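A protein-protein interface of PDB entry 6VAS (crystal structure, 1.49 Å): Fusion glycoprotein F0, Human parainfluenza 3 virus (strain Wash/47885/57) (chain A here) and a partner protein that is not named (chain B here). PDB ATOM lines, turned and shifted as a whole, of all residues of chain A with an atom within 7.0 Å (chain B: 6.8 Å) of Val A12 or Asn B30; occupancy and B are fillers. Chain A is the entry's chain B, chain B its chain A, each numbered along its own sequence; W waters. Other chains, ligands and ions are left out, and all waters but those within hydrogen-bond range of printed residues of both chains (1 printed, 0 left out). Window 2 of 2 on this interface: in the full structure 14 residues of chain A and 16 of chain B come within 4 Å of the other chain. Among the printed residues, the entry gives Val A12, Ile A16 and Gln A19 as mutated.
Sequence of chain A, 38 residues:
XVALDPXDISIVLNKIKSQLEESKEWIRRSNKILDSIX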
ATOM      1  N   ASP A   8     -26.490 -22.919  -5.386  1.00  0.00           N
ATOM      2  CA  ASP A   8     -26.316 -22.922  -6.834  1.00  0.00           C
ATOM      3  C   ASP A   8     -26.676 -21.555  -7.407  1.00  0.00           C
ATOM      4  O   ASP A   8     -25.829 -20.866  -7.976  1.00  0.00           O
ATOM      5  CB  ASP A   8     -27.184 -24.005  -7.474  1.00  0.00           C
ATOM      6  CG  ASP A   8     -26.963 -24.120  -8.971  1.00  0.00           C
ATOM      7  OD1 ASP A   8     -26.072 -23.423  -9.501  1.00  0.00           O
ATOM      8  OD2 ASP A   8     -27.682 -24.909  -9.618  1.00  0.00           O
ATOM      9  N   ILE A   9     -27.945 -21.169  -7.257  1.00  0.00           N
ATOM     10  CA  ILE A   9     -28.376 -19.860  -7.740  1.00  0.00           C
ATOM     11  C   ILE A   9     -27.743 -18.748  -6.916  1.00  0.00           C
ATOM     12  O   ILE A   9     -27.471 -17.658  -7.437  1.00  0.00           O
ATOM     13  CB  ILE A   9     -29.914 -19.775  -7.746  1.00  0.00           C
ATOM     14  CG1 ILE A   9     -30.488 -20.720  -8.804  1.00  0.00           C
ATOM     15  CG2 ILE A   9     -30.371 -18.346  -7.999  1.00  0.00           C
ATOM     16  CD1 ILE A   9     -31.784 -21.384  -8.392  1.00  0.00           C
ATOM     17  N   SER A  10     -27.491 -18.997  -5.629  1.00  0.00           N
ATOM     18  CA  SER A  10     -26.876 -17.976  -4.789  1.00  0.00           C
ATOM     19  C   SER A  10     -25.494 -17.602  -5.306  1.00  0.00           C
ATOM     20  O   SER A  10     -25.129 -16.420  -5.329  1.00  0.00           O
ATOM     21  CB  SER A  10     -26.793 -18.473  -3.347  1.00  0.00           C
ATOM     22  OG  SER A  10     -26.366 -17.438  -2.478  1.00  0.00           O
ATOM     23  N   ILE A  11     -24.708 -18.596  -5.725  1.00  0.00           N
ATOM     24  CA  ILE A  11     -23.387 -18.318  -6.282  1.00  0.00           C
ATOM     25  C   ILE A  11     -23.512 -17.486  -7.550  1.00  0.00           C
ATOM     26  O   ILE A  11     -22.749 -16.535  -7.766  1.00  0.00           O
ATOM     27  CB  ILE A  11     -22.627 -19.636  -6.531  1.00  0.00           C
ATOM     28  CG1 ILE A  11     -22.345 -20.342  -5.202  1.00  0.00           C
ATOM     29  CG2 ILE A  11     -21.334 -19.371  -7.289  1.00  0.00           C
ATOM     30  CD1 ILE A  11     -21.829 -21.760  -5.354  1.00  0.00           C
ATOM     31  N   VAL A  12     -24.473 -17.828  -8.411  1.00  0.00           N
ATOM     32  CA  VAL A  12     -24.645 -17.095  -9.662  1.00  0.00           C
ATOM     33  C   VAL A  12     -24.990 -15.638  -9.384  1.00  0.00           C
ATOM     34  O   VAL A  12     -24.466 -14.726 -10.033  1.00  0.00           O
ATOM     35  CB  VAL A  12     -25.702 -17.785 -10.544  1.00  0.00           C
ATOM     36  CG1 VAL A  12     -25.997 -16.941 -11.775  1.00  0.00           C
ATOM     37  CG2 VAL A  12     -25.235 -19.176 -10.939  1.00  0.00           C
ATOM     38  N   LEU A  13     -25.876 -15.391  -8.417  1.00  0.00           N
ATOM     39  CA  LEU A  13     -26.243 -14.016  -8.098  1.00  0.00           C
ATOM     40  C   LEU A  13     -25.076 -13.249  -7.483  1.00  0.00           C
ATOM     41  O   LEU A  13     -24.942 -12.043  -7.714  1.00  0.00           O
ATOM     42  CB  LEU A  13     -27.455 -13.997  -7.168  1.00  0.00           C
ATOM     43  CG  LEU A  13     -28.770 -14.477  -7.783  1.00  0.00           C
ATOM     44  CD1 LEU A  13     -29.872 -14.477  -6.730  1.00  0.00           C
ATOM     45  CD2 LEU A  13     -29.170 -13.625  -8.975  1.00  0.00           C
ATOM     46  N   ASN A  14     -24.223 -13.926  -6.711  1.00  0.00           N
ATOM     47  CA  ASN A  14     -23.045 -13.258  -6.160  1.00  0.00           C
ATOM     48  C   ASN A  14     -22.072 -12.854  -7.262  1.00  0.00           C
ATOM     49  O   ASN A  14     -21.466 -11.778  -7.198  1.00  0.00           O
ATOM     50  CB  ASN A  14     -22.356 -14.158  -5.133  1.00  0.00           C
ATOM     51  CG  ASN A  14     -22.988 -14.062  -3.759  1.00  0.00           C
ATOM     52  OD1 ASN A  14     -23.488 -13.009  -3.365  1.00  0.00           O
ATOM     53  ND2 ASN A  14     -22.968 -15.166  -3.020  1.00  0.00           N
ATOM     54  N   LYS A  15     -21.910 -13.702  -8.280  1.00  0.00           N
ATOM     55  CA  LYS A  15     -21.080 -13.327  -9.420  1.00  0.00           C
ATOM     56  C   LYS A  15     -21.612 -12.061 -10.081  1.00  0.00           C
ATOM     57  O   LYS A  15     -20.847 -11.144 -10.405  1.00  0.00           O
ATOM     58  CB  LYS A  15     -21.038 -14.461 -10.441  1.00  0.00           C
ATOM     59  CG  LYS A  15     -20.317 -15.717  -9.986  1.00  0.00           C
ATOM     60  CD  LYS A  15     -20.050 -16.622 -11.184  1.00  0.00           C
ATOM     61  CE  LYS A  15     -19.836 -18.070 -10.779  1.00  0.00           C
ATOM     62  NZ  LYS A  15     -19.822 -18.966 -11.972  1.00  0.00           N
ATOM     63  N   ILE A  16     -22.928 -11.998 -10.296  1.00  0.00           N
ATOM     64  CA  ILE A  16     -23.521 -10.823 -10.928  1.00  0.00           C
ATOM     65  C   ILE A  16     -23.233  -9.576 -10.102  1.00  0.00           C
ATOM     66  O   ILE A  16     -22.890  -8.517 -10.646  1.00  0.00           O
ATOM     67  CB  ILE A  16     -25.029 -11.037 -11.147  1.00  0.00           C
ATOM     68  CG1 ILE A  16     -25.269 -12.230 -12.075  1.00  0.00           C
ATOM     69  CG2 ILE A  16     -25.664  -9.778 -11.722  1.00  0.00           C
ATOM     70  CD1 ILE A  16     -26.708 -12.698 -12.113  1.00  0.00           C
ATOM     71  N   LYS A  17     -23.357  -9.682  -8.777  1.00  0.00           N
ATOM     72  CA  LYS A  17     -23.054  -8.549  -7.910  1.00  0.00           C
ATOM     73  C   LYS A  17     -21.606  -8.103  -8.080  1.00  0.00           C
ATOM     74  O   LYS A  17     -21.322  -6.906  -8.189  1.00  0.00           O
ATOM     75  CB  LYS A  17     -23.335  -8.914  -6.452  1.00  0.00           C
ATOM     76  CG  LYS A  17     -24.799  -8.842  -6.065  1.00  0.00           C
ATOM     77  CD  LYS A  17     -24.977  -9.005  -4.562  1.00  0.00           C
ATOM     78  CE  LYS A  17     -26.221  -8.278  -4.068  1.00  0.00           C
ATOM     79  NZ  LYS A  17     -26.395  -8.409  -2.594  1.00  0.00           N
ATOM     80  N   GLN A  19     -19.545  -8.647 -10.671  1.00  0.00           N
ATOM     81  CA  GLN A  19     -19.368  -8.064 -11.997  1.00  0.00           C
ATOM     82  C   GLN A  19     -20.002  -6.682 -12.087  1.00  0.00           C
ATOM     83  O   GLN A  19     -19.476  -5.799 -12.771  1.00  0.00           O
ATOM     84  CB  GLN A  19     -19.958  -9.002 -13.051  1.00  0.00           C
ATOM     85  CG  GLN A  19     -19.251 -10.339 -13.133  1.00  0.00           C
ATOM     86  CD  GLN A  19     -19.987 -11.343 -13.994  1.00  0.00           C
ATOM     87  OE1 GLN A  19     -21.216 -11.423 -13.964  1.00  0.00           O
ATOM     88  NE2 GLN A  19     -19.238 -12.120 -14.767  1.00  0.00           N
ATOM     89  N   GLN B  25     -22.148  -6.950 -19.792  1.00  0.00           N
ATOM     90  CA  GLN B  25     -22.457  -8.073 -20.672  1.00  0.00           C
ATOM     91  C   GLN B  25     -22.276  -9.398 -19.948  1.00  0.00           C
ATOM     92  O   GLN B  25     -23.102 -10.311 -20.089  1.00  0.00           O
ATOM     93  CB  GLN B  25     -21.568  -8.017 -21.913  1.00  0.00           C
ATOM     94  CG  GLN B  25     -21.890  -6.876 -22.862  1.00  0.00           C
ATOM     95  CD  GLN B  25     -20.782  -6.614 -23.867  1.00  0.00           C
ATOM     96  OE1 GLN B  25     -19.666  -7.124 -23.736  1.00  0.00           O
ATOM     97  NE2 GLN B  25     -21.086  -5.820 -24.882  1.00  0.00           N
ATOM     98  N   SER B  26     -21.194  -9.530 -19.178  1.00  0.00           N
ATOM     99  CA  SER B  26     -20.985 -10.753 -18.408  1.00  0.00           C
ATOM    100  C   SER B  26     -22.098 -10.943 -17.383  1.00  0.00           C
ATOM    101  O   SER B  26     -22.558 -12.069 -17.153  1.00  0.00           O
ATOM    102  CB  SER B  26     -19.623 -10.705 -17.718  1.00  0.00           C
ATOM    103  OG  SER B  26     -18.577 -10.542 -18.660  1.00  0.00           O
ATOM    104  N   SER B  27     -22.549  -9.848 -16.765  1.00  0.00           N
ATOM    105  CA  SER B  27     -23.643  -9.931 -15.805  1.00  0.00           C
ATOM    106  C   SER B  27     -24.920 -10.433 -16.465  1.00  0.00           C
ATOM    107  O   SER B  27     -25.649 -11.252 -15.888  1.00  0.00           O
ATOM    108  CB  SER B  27     -23.890  -8.559 -15.174  1.00  0.00           C
ATOM    109  OG  SER B  27     -22.787  -8.150 -14.388  1.00  0.00           O
ATOM    110  N   ILE B  28     -25.212  -9.953 -17.676  1.00  0.00           N
ATOM    111  CA  ILE B  28     -26.435 -10.366 -18.359  1.00  0.00           C
ATOM    112  C   ILE B  28     -26.382 -11.848 -18.706  1.00  0.00           C
ATOM    113  O   ILE B  28     -27.390 -12.560 -18.605  1.00  0.00           O
ATOM    114  CB  ILE B  28     -26.683  -9.479 -19.594  1.00  0.00           C
ATOM    115  CG1 ILE B  28     -27.138  -8.089 -19.143  1.00  0.00           C
ATOM    116  CG2 ILE B  28     -27.714 -10.120 -20.512  1.00  0.00           C
ATOM    117  CD1 ILE B  28     -27.047  -7.036 -20.217  1.00  0.00           C
ATOM    118  N   GLY B  29     -25.210 -12.338 -19.108  1.00  0.00           N
ATOM    119  CA  GLY B  29     -25.067 -13.765 -19.349  1.00  0.00           C
ATOM    120  C   GLY B  29     -25.392 -14.595 -18.123  1.00  0.00           C
ATOM    121  O   GLY B  29     -26.011 -15.658 -18.224  1.00  0.00           O
ATOM    122  N   ASN B  30     -24.991 -14.116 -16.943  1.00  0.00           N
ATOM    123  CA  ASN B  30     -25.272 -14.842 -15.709  1.00  0.00           C
ATOM    124  C   ASN B  30     -26.715 -14.663 -15.252  1.00  0.00           C
ATOM    125  O   ASN B  30     -27.268 -15.559 -14.604  1.00  0.00           O
ATOM    126  CB  ASN B  30     -24.305 -14.406 -14.607  1.00  0.00           C
ATOM    127  CG  ASN B  30     -22.957 -15.093 -14.709  1.00  0.00           C
ATOM    128  OD1 ASN B  30     -22.876 -16.294 -14.973  1.00  0.00           O
ATOM    129  ND2 ASN B  30     -21.886 -14.334 -14.503  1.00  0.00           N
ATOM    130  N   LEU B  31     -27.338 -13.525 -15.566  1.00  0.00           N
ATOM    131  CA  LEU B  31     -28.760 -13.368 -15.275  1.00  0.00           C
ATOM    132  C   LEU B  31     -29.585 -14.392 -16.047  1.00  0.00           C
ATOM    133  O   LEU B  31     -30.576 -14.923 -15.528  1.00  0.00           O
ATOM    134  CB  LEU B  31     -29.211 -11.948 -15.609  1.00  0.00           C
ATOM    135  CG  LEU B  31     -28.869 -10.876 -14.576  1.00  0.00           C
ATOM    136  CD1 LEU B  31     -29.080  -9.487 -15.164  1.00  0.00           C
ATOM    137  CD2 LEU B  31     -29.703 -11.048 -13.318  1.00  0.00           C
ATOM    138  N   ILE B  32     -29.186 -14.686 -17.287  1.00  0.00           N
ATOM    139  CA  ILE B  32     -29.842 -15.746 -18.046  1.00  0.00           C
ATOM    140  C   ILE B  32     -29.742 -17.067 -17.293  1.00  0.00           C
ATOM    141  O   ILE B  32     -30.736 -17.783 -17.117  1.00  0.00           O
ATOM    142  CB  ILE B  32     -29.231 -15.850 -19.457  1.00  0.00           C
ATOM    143  CG1 ILE B  32     -29.541 -14.592 -20.266  1.00  0.00           C
ATOM    144  CG2 ILE B  32     -29.753 -17.087 -20.168  1.00  0.00           C
ATOM    145  CD1 ILE B  32     -28.782 -14.510 -21.576  1.00  0.00           C
ATOM    146  N   VAL B  33     -28.534 -17.407 -16.837  1.00  0.00           N
ATOM    147  CA  VAL B  33     -28.340 -18.635 -16.071  1.00  0.00           C
ATOM    148  C   VAL B  33     -29.248 -18.653 -14.848  1.00  0.00           C
ATOM    149  O   VAL B  33     -29.870 -19.677 -14.533  1.00  0.00           O
ATOM    150  CB  VAL B  33     -26.856 -18.782 -15.684  1.00  0.00           C
ATOM    151  CG1 VAL B  33     -26.675 -19.901 -14.668  1.00  0.00           C
ATOM    152  CG2 VAL B  33     -26.006 -19.034 -16.921  1.00  0.00           C
ATOM    153  N   ALA B  34     -29.339 -17.523 -14.142  1.00  0.00           N
ATOM    154  CA  ALA B  34     -30.164 -17.468 -12.941  1.00  0.00           C
ATOM    155  C   ALA B  34     -31.633 -17.701 -13.266  1.00  0.00           C
ATOM    156  O   ALA B  34     -32.314 -18.465 -12.572  1.00  0.00           O
ATOM    157  CB  ALA B  34     -29.975 -16.121 -12.244  1.00  0.00           C
ATOM    158  N   ILE B  35     -32.136 -17.058 -14.321  1.00  0.00           N
ATOM    159  CA  ILE B  35     -33.537 -17.233 -14.696  1.00  0.00           C
ATOM    160  C   ILE B  35     -33.801 -18.679 -15.093  1.00  0.00           C
ATOM    161  O   ILE B  35     -34.782 -19.294 -14.652  1.00  0.00           O
ATOM    162  CB  ILE B  35     -33.920 -16.246 -15.814  1.00  0.00           C
ATOM    163  CG1 ILE B  35     -33.829 -14.810 -15.297  1.00  0.00           C
ATOM    164  CG2 ILE B  35     -35.318 -16.550 -16.326  1.00  0.00           C
ATOM    165  CD1 ILE B  35     -33.939 -13.756 -16.381  1.00  0.00           C
ATOM    166  N   SER B  37     -32.219 -21.280 -14.103  1.00  0.00           N
ATOM    167  CA  SER B  37     -32.147 -22.121 -12.914  1.00  0.00           C
ATOM    168  C   SER B  37     -33.479 -22.145 -12.174  1.00  0.00           C
ATOM    169  O   SER B  37     -33.997 -23.218 -11.840  1.00  0.00           O
ATOM    170  CB  SER B  37     -31.026 -21.634 -11.996  1.00  0.00           C
ATOM    171  OG  SER B  37     -29.756 -21.887 -12.574  1.00  0.00           O
HETATM  172  O   HOH W   1     -18.773 -15.376 -15.080  1.00  0.00           O
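N of Ser B27 lies close to OE1 of Gln A19 (3.5 Å).
The side-chain amide nitrogen of Asn B30 is in hydrogen-bond range of the side-chain amide oxygen of Gln A19, 3.0 Å away.
The side-chain hydroxyl of Ser B37 sits at hydrogen-bond distance from the backbone carbonyl oxygen of Val B33.
Among the printed residues, merely in contact across the chains: Gln A19 with Ser B26, Ile A9 with Ser B37, Val A12 with Asn B30, Ile A16 with Asn B30, Ile A16 with Leu B31 and Ile A16 with Ser B27.
Val A12 touches just one residue of chain B: Asn B30 (3.4 Å).
Of chain A, only Val A12, Ile A16 and Gln A19 come within 4 Å of Asn B30.
No residue of chain A comes within 4 Å of Gly B29.
Printed residues of chain A within 4 Å of Leu B31: Ile A16 (3.6 Å).
Of the printed residues of chain A, Ser B27 touches Ile A16 and Gln A19.
Of the printed residues of chain B, Ile A9 touches Ser B37.
Of the printed residues of chain B, Ile A16 touches Ser B27, Asn B30 and Leu B31.
Of the printed residues of chain B, Gln A19 touches Ser B26, Ser B27 and Asn B30.
Ala B34 touches none of the printed residues of chain A.
The nearest printed residue of chain A that does not touch Ser B26 is Ile A16 (5.8 Å).
Of the 12 printed residues of chain B, 5 touch a printed residue of chain A.
Printed residues of chain B that touch a printed residue of chain A: Ser B26, Ser B27, Asn B30, Leu B31 and Ser B37.
Printed residues of chain A that touch a printed residue of chain B: Ile A9, Val A12, Ile A16 and Gln A19.
Hydrophobic or aromatic side chains of chain A that line the printed part of chain B: Ile A9, Val A12 and Ile A16.
Among the printed residues, no Asp or Glu carboxylate lies within 4 Å of a Lys or Arg side-chain nitrogen of the other chain.
Water W1 bridges the side-chain amide nitrogen (NE2) of Gln A19 (3.3 Å) and the side-chain amide nitrogen (ND2) of Asn B30 (3.3 Å).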
